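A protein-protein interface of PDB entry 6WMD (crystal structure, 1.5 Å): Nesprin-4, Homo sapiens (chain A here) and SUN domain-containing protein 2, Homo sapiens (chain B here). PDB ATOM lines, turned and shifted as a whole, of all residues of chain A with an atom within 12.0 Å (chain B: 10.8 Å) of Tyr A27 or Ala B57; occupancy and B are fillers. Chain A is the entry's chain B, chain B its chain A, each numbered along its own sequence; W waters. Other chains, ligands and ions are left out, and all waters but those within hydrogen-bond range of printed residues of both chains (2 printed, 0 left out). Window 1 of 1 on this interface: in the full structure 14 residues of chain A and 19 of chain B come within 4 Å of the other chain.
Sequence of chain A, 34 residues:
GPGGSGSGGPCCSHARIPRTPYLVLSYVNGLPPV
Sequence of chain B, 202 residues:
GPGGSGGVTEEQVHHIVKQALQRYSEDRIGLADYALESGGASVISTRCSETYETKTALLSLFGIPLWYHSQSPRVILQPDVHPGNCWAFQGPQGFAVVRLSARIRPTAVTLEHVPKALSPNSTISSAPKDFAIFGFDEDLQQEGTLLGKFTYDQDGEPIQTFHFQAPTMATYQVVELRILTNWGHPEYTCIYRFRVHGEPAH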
ATOM      1  N   LEU A  23      -0.694  -7.721  -0.312  1.00  0.00           N
ATOM      2  CA  LEU A  23      -0.619  -9.133  -0.662  1.00  0.00           C
ATOM      3  C   LEU A  23      -1.918  -9.528  -1.358  1.00  0.00           C
ATOM      4  O   LEU A  23      -3.002  -9.362  -0.793  1.00  0.00           O
ATOM      5  CB  LEU A  23      -0.422  -9.976   0.594  1.00  0.00           C
ATOM      6  CG  LEU A  23       0.656 -11.061   0.542  1.00  0.00           C
ATOM      7  CD1 LEU A  23       1.951 -10.541  -0.068  1.00  0.00           C
ATOM      8  CD2 LEU A  23       0.901 -11.617   1.934  1.00  0.00           C
ATOM      9  N   VAL A  24      -1.810 -10.021  -2.589  1.00  0.00           N
ATOM     10  CA  VAL A  24      -2.968 -10.398  -3.396  1.00  0.00           C
ATOM     11  C   VAL A  24      -3.140 -11.906  -3.290  1.00  0.00           C
ATOM     12  O   VAL A  24      -2.164 -12.655  -3.373  1.00  0.00           O
ATOM     13  CB  VAL A  24      -2.749  -9.968  -4.862  1.00  0.00           C
ATOM     14  CG1 VAL A  24      -3.789 -10.604  -5.785  1.00  0.00           C
ATOM     15  CG2 VAL A  24      -2.770  -8.453  -4.982  1.00  0.00           C
ATOM     16  N   LEU A  25      -4.382 -12.364  -3.126  1.00  0.00           N
ATOM     17  CA  LEU A  25      -4.677 -13.792  -3.050  1.00  0.00           C
ATOM     18  C   LEU A  25      -5.625 -14.158  -4.181  1.00  0.00           C
ATOM     19  O   LEU A  25      -6.732 -13.615  -4.261  1.00  0.00           O
ATOM     20  CB  LEU A  25      -5.316 -14.153  -1.708  1.00  0.00           C
ATOM     21  CG  LEU A  25      -5.874 -15.578  -1.657  1.00  0.00           C
ATOM     22  CD1 LEU A  25      -4.741 -16.585  -1.683  1.00  0.00           C
ATOM     23  CD2 LEU A  25      -6.741 -15.794  -0.426  1.00  0.00           C
ATOM     24  N   SER A  26      -5.196 -15.083  -5.047  1.00  0.00           N
ATOM     25  CA  SER A  26      -6.009 -15.557  -6.156  1.00  0.00           C
ATOM     26  C   SER A  26      -6.070 -17.073  -6.096  1.00  0.00           C
ATOM     27  O   SER A  26      -5.072 -17.728  -5.794  1.00  0.00           O
ATOM     28  CB  SER A  26      -5.423 -15.138  -7.506  1.00  0.00           C
ATOM     29  OG  SER A  26      -5.111 -13.757  -7.521  1.00  0.00           O
ATOM     30  N   TYR A  27      -7.249 -17.627  -6.372  1.00  0.00           N
ATOM     31  CA  TYR A  27      -7.424 -19.076  -6.440  1.00  0.00           C
ATOM     32  C   TYR A  27      -7.265 -19.514  -7.888  1.00  0.00           C
ATOM     33  O   TYR A  27      -8.092 -19.177  -8.743  1.00  0.00           O
ATOM     34  CB  TYR A  27      -8.785 -19.480  -5.885  1.00  0.00           C
ATOM     35  CG  TYR A  27      -8.846 -19.379  -4.382  1.00  0.00           C
ATOM     36  CD1 TYR A  27      -8.337 -20.393  -3.577  1.00  0.00           C
ATOM     37  CD2 TYR A  27      -9.384 -18.260  -3.763  1.00  0.00           C
ATOM     38  CE1 TYR A  27      -8.369 -20.300  -2.203  1.00  0.00           C
ATOM     39  CE2 TYR A  27      -9.432 -18.164  -2.386  1.00  0.00           C
ATOM     40  CZ  TYR A  27      -8.920 -19.178  -1.608  1.00  0.00           C
ATOM     41  OH  TYR A  27      -8.963 -19.093  -0.229  1.00  0.00           O
ATOM     42  N   VAL A  28      -6.209 -20.275  -8.160  1.00  0.00           N
ATOM     43  CA  VAL A  28      -5.839 -20.635  -9.526  1.00  0.00           C
ATOM     44  C   VAL A  28      -6.082 -22.100  -9.852  1.00  0.00           C
ATOM     45  O   VAL A  28      -5.920 -22.492 -11.020  1.00  0.00           O
ATOM     46  CB  VAL A  28      -4.381 -20.239  -9.844  1.00  0.00           C
ATOM     47  CG1 VAL A  28      -4.175 -18.759  -9.578  1.00  0.00           C
ATOM     48  CG2 VAL A  28      -3.423 -21.071  -9.016  1.00  0.00           C
ATOM     49  N   ASN A  29      -6.473 -22.917  -8.875  1.00  0.00           N
ATOM     50  CA  ASN A  29      -6.658 -24.353  -9.062  1.00  0.00           C
ATOM     51  C   ASN A  29      -7.866 -24.847  -8.271  1.00  0.00           C
ATOM     52  O   ASN A  29      -7.817 -25.890  -7.609  1.00  0.00           O
ATOM     53  CB  ASN A  29      -5.390 -25.124  -8.684  1.00  0.00           C
ATOM     54  CG  ASN A  29      -5.440 -26.585  -9.100  1.00  0.00           C
ATOM     55  OD1 ASN A  29      -6.041 -26.935 -10.117  1.00  0.00           O
ATOM     56  ND2 ASN A  29      -4.811 -27.446  -8.308  1.00  0.00           N
ATOM     57  N   GLY A  30      -8.964 -24.099  -8.322  1.00  0.00           N
ATOM     58  CA  GLY A  30     -10.192 -24.547  -7.687  1.00  0.00           C
ATOM     59  C   GLY A  30     -10.233 -24.311  -6.186  1.00  0.00           C
ATOM     60  O   GLY A  30      -9.493 -23.504  -5.613  1.00  0.00           O
ATOM     61  N   LEU A  31     -11.127 -25.053  -5.547  1.00  0.00           N
ATOM     62  CA  LEU A  31     -11.468 -24.798  -4.155  1.00  0.00           C
ATOM     63  C   LEU A  31     -10.345 -25.230  -3.213  1.00  0.00           C
ATOM     64  O   LEU A  31      -9.684 -26.251  -3.437  1.00  0.00           O
ATOM     65  CB  LEU A  31     -12.727 -25.572  -3.775  1.00  0.00           C
ATOM     66  CG  LEU A  31     -14.072 -25.036  -4.267  1.00  0.00           C
ATOM     67  CD1 LEU A  31     -15.129 -26.111  -4.153  1.00  0.00           C
ATOM     68  CD2 LEU A  31     -14.493 -23.815  -3.445  1.00  0.00           C
ATOM     69  N   PRO A  32     -10.141 -24.496  -2.128  1.00  0.00           N
ATOM     70  CA  PRO A  32      -9.313 -25.003  -1.044  1.00  0.00           C
ATOM     71  C   PRO A  32     -10.105 -26.024  -0.253  1.00  0.00           C
ATOM     72  O   PRO A  32     -11.333 -26.106  -0.414  1.00  0.00           O
ATOM     73  CB  PRO A  32      -9.056 -23.747  -0.201  1.00  0.00           C
ATOM     74  CG  PRO A  32     -10.336 -22.944  -0.365  1.00  0.00           C
ATOM     75  CD  PRO A  32     -10.818 -23.229  -1.782  1.00  0.00           C
ATOM     76  N   PRO A  33      -9.466 -26.804   0.618  1.00  0.00           N
ATOM     77  CA  PRO A  33     -10.233 -27.747   1.446  1.00  0.00           C
ATOM     78  C   PRO A  33     -11.146 -27.004   2.412  1.00  0.00           C
ATOM     79  O   PRO A  33     -10.759 -26.003   3.024  1.00  0.00           O
ATOM     80  CB  PRO A  33      -9.143 -28.528   2.194  1.00  0.00           C
ATOM     81  CG  PRO A  33      -7.907 -28.360   1.333  1.00  0.00           C
ATOM     82  CD  PRO A  33      -8.015 -26.955   0.819  1.00  0.00           C
ATOM     83  N   VAL A  34     -12.382 -27.492   2.529  1.00  0.00           N
ATOM     84  CA  VAL A  34     -13.382 -26.872   3.401  1.00  0.00           C
ATOM     85  C   VAL A  34     -14.117 -27.979   4.137  1.00  0.00           C
ATOM     86  O   VAL A  34     -14.540 -27.830   5.299  1.00  0.00           O
ATOM     87  CB  VAL A  34     -14.370 -26.016   2.580  1.00  0.00           C
ATOM     88  CG1 VAL A  34     -15.528 -25.538   3.437  1.00  0.00           C
ATOM     89  CG2 VAL A  34     -13.656 -24.842   1.920  1.00  0.00           C
ATOM     90  OXT VAL A  34     -14.309 -29.054   3.555  1.00  0.00           O
ATOM     91  N   TYR B  52      -2.454 -31.939   3.483  1.00  0.00           N
ATOM     92  CA  TYR B  52      -2.948 -32.011   2.114  1.00  0.00           C
ATOM     93  C   TYR B  52      -2.791 -30.629   1.484  1.00  0.00           C
ATOM     94  O   TYR B  52      -3.360 -29.656   1.984  1.00  0.00           O
ATOM     95  CB  TYR B  52      -4.434 -32.369   2.190  1.00  0.00           C
ATOM     96  CG  TYR B  52      -5.147 -32.532   0.861  1.00  0.00           C
ATOM     97  CD1 TYR B  52      -5.158 -33.750   0.201  1.00  0.00           C
ATOM     98  CD2 TYR B  52      -5.835 -31.475   0.285  1.00  0.00           C
ATOM     99  CE1 TYR B  52      -5.823 -33.908  -1.003  1.00  0.00           C
ATOM    100  CE2 TYR B  52      -6.499 -31.624  -0.915  1.00  0.00           C
ATOM    101  CZ  TYR B  52      -6.490 -32.839  -1.555  1.00  0.00           C
ATOM    102  OH  TYR B  52      -7.150 -32.977  -2.757  1.00  0.00           O
ATOM    103  N   GLU B  53      -2.030 -30.519   0.409  1.00  0.00           N
ATOM    104  CA  GLU B  53      -1.865 -29.229  -0.252  1.00  0.00           C
ATOM    105  C   GLU B  53      -2.479 -29.264  -1.642  1.00  0.00           C
ATOM    106  O   GLU B  53      -2.217 -30.186  -2.420  1.00  0.00           O
ATOM    107  CB  GLU B  53      -0.405 -28.780  -0.287  1.00  0.00           C
ATOM    108  CG  GLU B  53       0.191 -28.603   1.096  1.00  0.00           C
ATOM    109  CD  GLU B  53       1.699 -28.687   1.091  1.00  0.00           C
ATOM    110  OE1 GLU B  53       2.333 -28.226   2.064  1.00  0.00           O
ATOM    111  OE2 GLU B  53       2.251 -29.194   0.093  1.00  0.00           O
ATOM    112  N   THR B  54      -3.320 -28.271  -1.929  1.00  0.00           N
ATOM    113  CA  THR B  54      -4.047 -28.192  -3.186  1.00  0.00           C
ATOM    114  C   THR B  54      -3.327 -27.364  -4.239  1.00  0.00           C
ATOM    115  O   THR B  54      -3.651 -27.486  -5.425  1.00  0.00           O
ATOM    116  CB  THR B  54      -5.421 -27.556  -2.948  1.00  0.00           C
ATOM    117  OG1 THR B  54      -5.272 -26.413  -2.094  1.00  0.00           O
ATOM    118  CG2 THR B  54      -6.364 -28.542  -2.290  1.00  0.00           C
ATOM    119  N   LYS B  55      -2.376 -26.524  -3.835  1.00  0.00           N
ATOM    120  CA  LYS B  55      -1.713 -25.592  -4.744  1.00  0.00           C
ATOM    121  C   LYS B  55      -2.730 -24.728  -5.487  1.00  0.00           C
ATOM    122  O   LYS B  55      -2.727 -24.633  -6.717  1.00  0.00           O
ATOM    123  CB  LYS B  55      -0.779 -26.315  -5.718  1.00  0.00           C
ATOM    124  CG  LYS B  55       0.414 -26.993  -5.061  1.00  0.00           C
ATOM    125  CD  LYS B  55       1.115 -26.051  -4.109  1.00  0.00           C
ATOM    126  CE  LYS B  55       2.183 -26.756  -3.295  1.00  0.00           C
ATOM    127  NZ  LYS B  55       1.980 -26.498  -1.843  1.00  0.00           N
ATOM    128  N   THR B  56      -3.614 -24.089  -4.726  1.00  0.00           N
ATOM    129  CA  THR B  56      -4.605 -23.220  -5.347  1.00  0.00           C
ATOM    130  C   THR B  56      -4.565 -21.780  -4.862  1.00  0.00           C
ATOM    131  O   THR B  56      -4.711 -20.867  -5.675  1.00  0.00           O
ATOM    132  CB  THR B  56      -6.028 -23.793  -5.226  1.00  0.00           C
ATOM    133  OG1 THR B  56      -6.921 -22.960  -5.975  1.00  0.00           O
ATOM    134  CG2 THR B  56      -6.494 -23.875  -3.764  1.00  0.00           C
ATOM    135  N   ALA B  57      -4.353 -21.544  -3.569  1.00  0.00           N
ATOM    136  CA  ALA B  57      -4.409 -20.189  -3.015  1.00  0.00           C
ATOM    137  C   ALA B  57      -3.051 -19.528  -3.223  1.00  0.00           C
ATOM    138  O   ALA B  57      -2.135 -19.670  -2.411  1.00  0.00           O
ATOM    139  CB  ALA B  57      -4.782 -20.236  -1.540  1.00  0.00           C
ATOM    140  N   LEU B  58      -2.919 -18.790  -4.323  1.00  0.00           N
ATOM    141  CA  LEU B  58      -1.644 -18.192  -4.703  1.00  0.00           C
ATOM    142  C   LEU B  58      -1.557 -16.777  -4.143  1.00  0.00           C
ATOM    143  O   LEU B  58      -2.429 -15.942  -4.409  1.00  0.00           O
ATOM    144  CB  LEU B  58      -1.502 -18.175  -6.225  1.00  0.00           C
ATOM    145  CG  LEU B  58      -0.247 -17.516  -6.796  1.00  0.00           C
ATOM    146  CD1 LEU B  58       0.998 -18.222  -6.291  1.00  0.00           C
ATOM    147  CD2 LEU B  58      -0.293 -17.528  -8.313  1.00  0.00           C
ATOM    148  N   LEU B  59      -0.511 -16.511  -3.366  1.00  0.00           N
ATOM    149  CA  LEU B  59      -0.241 -15.173  -2.867  1.00  0.00           C
ATOM    150  C   LEU B  59       0.763 -14.493  -3.782  1.00  0.00           C
ATOM    151  O   LEU B  59       1.744 -15.107  -4.211  1.00  0.00           O
ATOM    152  CB  LEU B  59       0.305 -15.212  -1.440  1.00  0.00           C
ATOM    153  CG  LEU B  59      -0.734 -15.660  -0.419  1.00  0.00           C
ATOM    154  CD1 LEU B  59      -0.063 -16.277   0.795  1.00  0.00           C
ATOM    155  CD2 LEU B  59      -1.628 -14.484  -0.035  1.00  0.00           C
ATOM    156  N   SER B  60       0.505 -13.229  -4.093  1.00  0.00           N
ATOM    157  CA  SER B  60       1.387 -12.469  -4.960  1.00  0.00           C
ATOM    158  C   SER B  60       1.598 -11.078  -4.385  1.00  0.00           C
ATOM    159  O   SER B  60       0.820 -10.590  -3.563  1.00  0.00           O
ATOM    160  CB  SER B  60       0.865 -12.392  -6.402  1.00  0.00           C
ATOM    161  OG  SER B  60      -0.345 -11.662  -6.469  1.00  0.00           O
ATOM    162  N   LEU B  61       2.695 -10.454  -4.821  1.00  0.00           N
ATOM    163  CA  LEU B  61       3.063  -9.113  -4.393  1.00  0.00           C
ATOM    164  C   LEU B  61       3.685  -8.401  -5.583  1.00  0.00           C
ATOM    165  O   LEU B  61       4.577  -8.952  -6.236  1.00  0.00           O
ATOM    166  CB  LEU B  61       4.066  -9.168  -3.238  1.00  0.00           C
ATOM    167  CG  LEU B  61       4.531  -7.815  -2.703  1.00  0.00           C
ATOM    168  CD1 LEU B  61       3.340  -6.977  -2.276  1.00  0.00           C
ATOM    169  CD2 LEU B  61       5.498  -8.009  -1.547  1.00  0.00           C
ATOM    170  N   ILE B  64       4.173 -10.386  -8.546  1.00  0.00           N
ATOM    171  CA  ILE B  64       5.102 -11.512  -8.477  1.00  0.00           C
ATOM    172  C   ILE B  64       4.430 -12.628  -7.685  1.00  0.00           C
ATOM    173  O   ILE B  64       4.121 -12.430  -6.502  1.00  0.00           O
ATOM    174  CB  ILE B  64       6.423 -11.098  -7.817  1.00  0.00           C
ATOM    175  CG1 ILE B  64       7.153 -10.065  -8.676  1.00  0.00           C
ATOM    176  CG2 ILE B  64       7.306 -12.315  -7.583  1.00  0.00           C
ATOM    177  CD1 ILE B  64       7.768  -8.934  -7.875  1.00  0.00           C
ATOM    178  N   PRO B  65       4.204 -13.801  -8.276  1.00  0.00           N
ATOM    179  CA  PRO B  65       3.711 -14.941  -7.492  1.00  0.00           C
ATOM    180  C   PRO B  65       4.748 -15.371  -6.463  1.00  0.00           C
ATOM    181  O   PRO B  65       5.915 -15.590  -6.792  1.00  0.00           O
ATOM    182  CB  PRO B  65       3.486 -16.027  -8.550  1.00  0.00           C
ATOM    183  CG  PRO B  65       4.395 -15.640  -9.687  1.00  0.00           C
ATOM    184  CD  PRO B  65       4.410 -14.143  -9.694  1.00  0.00           C
ATOM    185  N   LEU B  66       4.312 -15.487  -5.209  1.00  0.00           N
ATOM    186  CA  LEU B  66       5.205 -15.820  -4.103  1.00  0.00           C
ATOM    187  C   LEU B  66       5.131 -17.299  -3.741  1.00  0.00           C
ATOM    188  O   LEU B  66       6.081 -18.050  -3.986  1.00  0.00           O
ATOM    189  CB  LEU B  66       4.882 -14.970  -2.874  1.00  0.00           C
ATOM    190  CG  LEU B  66       4.894 -13.454  -3.052  1.00  0.00           C
ATOM    191  CD1 LEU B  66       4.516 -12.774  -1.750  1.00  0.00           C
ATOM    192  CD2 LEU B  66       6.260 -12.996  -3.515  1.00  0.00           C
ATOM    193  N   TRP B  67       4.023 -17.724  -3.138  1.00  0.00           N
ATOM    194  CA  TRP B  67       3.844 -19.127  -2.792  1.00  0.00           C
ATOM    195  C   TRP B  67       2.357 -19.412  -2.661  1.00  0.00           C
ATOM    196  O   TRP B  67       1.523 -18.504  -2.667  1.00  0.00           O
ATOM    197  CB  TRP B  67       4.562 -19.487  -1.485  1.00  0.00           C
ATOM    198  CG  TRP B  67       4.101 -18.666  -0.325  1.00  0.00           C
ATOM    199  CD1 TRP B  67       2.944 -18.820   0.391  1.00  0.00           C
ATOM    200  CD2 TRP B  67       4.782 -17.549   0.250  1.00  0.00           C
ATOM    201  NE1 TRP B  67       2.868 -17.865   1.377  1.00  0.00           N
ATOM    202  CE2 TRP B  67       3.986 -17.074   1.312  1.00  0.00           C
ATOM    203  CE3 TRP B  67       5.991 -16.907  -0.027  1.00  0.00           C
ATOM    204  CZ2 TRP B  67       4.360 -15.986   2.094  1.00  0.00           C
ATOM    205  CZ3 TRP B  67       6.360 -15.827   0.751  1.00  0.00           C
ATOM    206  CH2 TRP B  67       5.548 -15.377   1.798  1.00  0.00           C
ATOM    207  N   TYR B  68       2.040 -20.696  -2.528  1.00  0.00           N
ATOM    208  CA  TYR B  68       0.678 -21.130  -2.269  1.00  0.00           C
ATOM    209  C   TYR B  68       0.446 -21.203  -0.769  1.00  0.00           C
ATOM    210  O   TYR B  68       1.326 -21.615  -0.011  1.00  0.00           O
ATOM    211  CB  TYR B  68       0.422 -22.496  -2.901  1.00  0.00           C
ATOM    212  CG  TYR B  68       0.409 -22.456  -4.411  1.00  0.00           C
ATOM    213  CD1 TYR B  68       1.504 -22.883  -5.149  1.00  0.00           C
ATOM    214  CD2 TYR B  68      -0.701 -21.982  -5.098  1.00  0.00           C
ATOM    215  CE1 TYR B  68       1.492 -22.848  -6.525  1.00  0.00           C
ATOM    216  CE2 TYR B  68      -0.723 -21.940  -6.475  1.00  0.00           C
ATOM    217  CZ  TYR B  68       0.375 -22.374  -7.183  1.00  0.00           C
ATOM    218  OH  TYR B  68       0.360 -22.336  -8.557  1.00  0.00           O
ATOM    219  N   HIS B  69      -0.737 -20.789  -0.345  1.00  0.00           N
ATOM    220  CA  HIS B  69      -1.074 -20.768   1.070  1.00  0.00           C
ATOM    221  C   HIS B  69      -1.950 -21.964   1.423  1.00  0.00           C
ATOM    222  O   HIS B  69      -2.987 -22.191   0.792  1.00  0.00           O
ATOM    223  CB  HIS B  69      -1.803 -19.474   1.424  1.00  0.00           C
ATOM    224  CG  HIS B  69      -2.414 -19.492   2.788  1.00  0.00           C
ATOM    225  ND1 HIS B  69      -1.690 -19.219   3.928  1.00  0.00           N
ATOM    226  CD2 HIS B  69      -3.673 -19.774   3.198  1.00  0.00           C
ATOM    227  CE1 HIS B  69      -2.479 -19.321   4.982  1.00  0.00           C
ATOM    228  NE2 HIS B  69      -3.688 -19.656   4.568  1.00  0.00           N
ATOM    229  N   SER B  70      -1.513 -22.735   2.418  1.00  0.00           N
ATOM    230  CA  SER B  70      -2.310 -23.797   3.018  1.00  0.00           C
ATOM    231  C   SER B  70      -2.207 -23.669   4.530  1.00  0.00           C
ATOM    232  O   SER B  70      -1.189 -23.214   5.055  1.00  0.00           O
ATOM    233  CB  SER B  70      -1.807 -25.197   2.609  1.00  0.00           C
ATOM    234  OG  SER B  70      -2.086 -25.496   1.245  1.00  0.00           O
ATOM    235  N   GLN B  71      -3.261 -24.079   5.225  1.00  0.00           N
ATOM    236  CA  GLN B  71      -3.257 -24.032   6.677  1.00  0.00           C
ATOM    237  C   GLN B  71      -2.447 -25.196   7.231  1.00  0.00           C
ATOM    238  O   GLN B  71      -2.562 -26.330   6.759  1.00  0.00           O
ATOM    239  CB  GLN B  71      -4.687 -24.125   7.211  1.00  0.00           C
ATOM    240  CG  GLN B  71      -5.680 -23.178   6.533  1.00  0.00           C
ATOM    241  CD  GLN B  71      -5.429 -21.722   6.873  1.00  0.00           C
ATOM    242  OE1 GLN B  71      -4.760 -21.406   7.856  1.00  0.00           O
ATOM    243  NE2 GLN B  71      -5.969 -20.826   6.059  1.00  0.00           N
ATOM    244  N   HIS B  82     -14.087 -20.520  10.507  1.00  0.00           N
ATOM    245  CA  HIS B  82     -14.853 -20.078   9.358  1.00  0.00           C
ATOM    246  C   HIS B  82     -14.512 -21.038   8.235  1.00  0.00           C
ATOM    247  O   HIS B  82     -13.416 -21.610   8.229  1.00  0.00           O
ATOM    248  CB  HIS B  82     -14.424 -18.673   8.920  1.00  0.00           C
ATOM    249  CG  HIS B  82     -14.685 -17.634   9.957  1.00  0.00           C
ATOM    250  ND1 HIS B  82     -15.938 -17.096  10.166  1.00  0.00           N
ATOM    251  CD2 HIS B  82     -13.867 -17.066  10.873  1.00  0.00           C
ATOM    252  CE1 HIS B  82     -15.872 -16.220  11.156  1.00  0.00           C
ATOM    253  NE2 HIS B  82     -14.628 -16.183  11.603  1.00  0.00           N
ATOM    254  N   PRO B  83     -15.416 -21.228   7.274  1.00  0.00           N
ATOM    255  CA  PRO B  83     -15.160 -22.188   6.186  1.00  0.00           C
ATOM    256  C   PRO B  83     -13.790 -22.002   5.551  1.00  0.00           C
ATOM    257  O   PRO B  83     -13.411 -20.899   5.151  1.00  0.00           O
ATOM    258  CB  PRO B  83     -16.282 -21.886   5.189  1.00  0.00           C
ATOM    259  CG  PRO B  83     -17.421 -21.430   6.077  1.00  0.00           C
ATOM    260  CD  PRO B  83     -16.767 -20.650   7.193  1.00  0.00           C
ATOM    261  N   GLY B  84     -13.029 -23.099   5.476  1.00  0.00           N
ATOM    262  CA  GLY B  84     -11.702 -23.062   4.878  1.00  0.00           C
ATOM    263  C   GLY B  84     -10.571 -22.792   5.851  1.00  0.00           C
ATOM    264  O   GLY B  84      -9.404 -23.025   5.502  1.00  0.00           O
ATOM    265  N   ASN B  85     -10.884 -22.293   7.050  1.00  0.00           N
ATOM    266  CA  ASN B  85      -9.908 -22.105   8.125  1.00  0.00           C
ATOM    267  C   ASN B  85      -9.796 -23.413   8.900  1.00  0.00           C
ATOM    268  O   ASN B  85     -10.193 -23.532  10.061  1.00  0.00           O
ATOM    269  CB  ASN B  85     -10.364 -21.004   9.071  1.00  0.00           C
ATOM    270  CG  ASN B  85     -10.256 -19.628   8.471  1.00  0.00           C
ATOM    271  OD1 ASN B  85      -9.753 -19.439   7.362  1.00  0.00           O
ATOM    272  ND2 ASN B  85     -10.738 -18.640   9.215  1.00  0.00           N
ATOM    273  N   CYS B  86      -9.271 -24.416   8.213  1.00  0.00           N
ATOM    274  CA  CYS B  86      -9.176 -25.737   8.794  1.00  0.00           C
ATOM    275  C   CYS B  86      -7.881 -26.343   8.288  1.00  0.00           C
ATOM    276  O   CYS B  86      -7.311 -25.889   7.284  1.00  0.00           O
ATOM    277  CB  CYS B  86     -10.333 -26.646   8.335  1.00  0.00           C
ATOM    278  SG  CYS B  86     -10.742 -26.489   6.560  1.00  0.00           S
HETATM  279  O   HOH W   1      -2.124 -13.950  -6.484  1.00  0.00           O
HETATM  280  O   HOH W   2      -8.545 -24.525   3.459  1.00  0.00           O
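Water W2 bridges O of Gly B84 (2.7 Å) and O of Pro A33 (2.7 Å). Water W1 lies within hydrogen-bond range of O of Leu B58 (2.9 Å), OG of Ser B60 (2.9 Å), OG of Ser A26 (3.2 Å) and O of Val A24 (3.4 Å).
Tyr A27 touches just these residues of chain B: Thr B56 and Ala B57. Of the printed residues of chain B, Val A28 touches Thr B56 (3.0 Å) and Tyr B68 (3.8 Å). Printed residues of chain B within 4 Å of Val A34: Gly B84. Of the printed residues of chain A, Tyr B52 touches Pro A33. Of chain A, only Asn A29 and Pro A33 come within 4 Å of Thr B54. Of the printed residues of chain A, Ala B57 touches Leu A25 (3.7 Å), Ser A26 (3.7 Å) and Tyr A27 (3.6 Å). Leu B59 touches just one residue of chain A: Val A24. Of the printed residues of chain A, Leu B66 touches Leu A23. Of chain A, only Val A28 comes within 4 Å of Tyr B68. Ser B70 touches none of the printed residues of chain A.
N of Leu B59 sits at hydrogen-bond distance from O of Trp B67. N of Leu B66 lies within hydrogen-bond range of O of Leu B59 (2.8 Å). OE2 of Glu B53 is in salt-bridge range of NZ of Lys B55, at 3.3 Å. The backbone carbonyl oxygen of Ala B57 is in hydrogen-bond range of the backbone NH of His B69, 2.7 Å away.
The backbone carbonyl oxygen of Ser A26 lies close to the backbone carbonyl oxygen of Thr B56 (3.2 Å). The backbone carbonyl oxygen (O) of Thr B56 lies within hydrogen-bond range of the backbone NH (N) of Val A28 (3.0 Å). N of Leu B58 lies within hydrogen-bond range of O of Ser A26, 2.8 Å away. The side-chain sulfur (SG) of Cys B86 sits at hydrogen-bond distance from the backbone carbonyl oxygen (O) of Pro A33, at 3.6 Å. O of Val A24 sits at hydrogen-bond distance from N of Ser B60 (2.8 Å). O of Val A24 sits close to O of Leu B58 (3.5 Å). The side-chain amide nitrogen (ND2) of Asn A29 lies within hydrogen-bond range of the backbone carbonyl oxygen (O) of Thr B54 (3.1 Å). OG1 of Thr B56 sits at hydrogen-bond distance from N of Asn A29. The backbone carbonyl oxygen (O) of Gly A30 is in hydrogen-bond range of the side-chain hydroxyl (OG1) of Thr B56, at 2.7 Å.
Printed residues of chain A that touch a printed residue of chain B: Leu A23, Val A24, Leu A25, Ser A26, Tyr A27, Val A28, Asn A29, Gly A30, Leu A31, Pro A33 and Val A34. Of the 23 printed residues of chain B, 12 touch a printed residue of chain A. Among the printed residues, 24 pairs touch across the chains.
Among the printed residues, merely in contact across the chains: Val A24 with Leu B59, Tyr A27 with Thr B56, Asn A29 with Lys B55, Leu A25 with Leu B58, Leu A23 with Ser B60, Pro A33 with Gly B84, Tyr A27 with Ala B57, Leu A25 with Ala B57, Ser A26 with Ala B57, Leu A23 with Leu B66, Val A28 with Tyr B68, Pro A33 with Thr B54, Pro A33 with Tyr B52, Val A34 with Gly B84 and Leu A31 with Thr B56.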
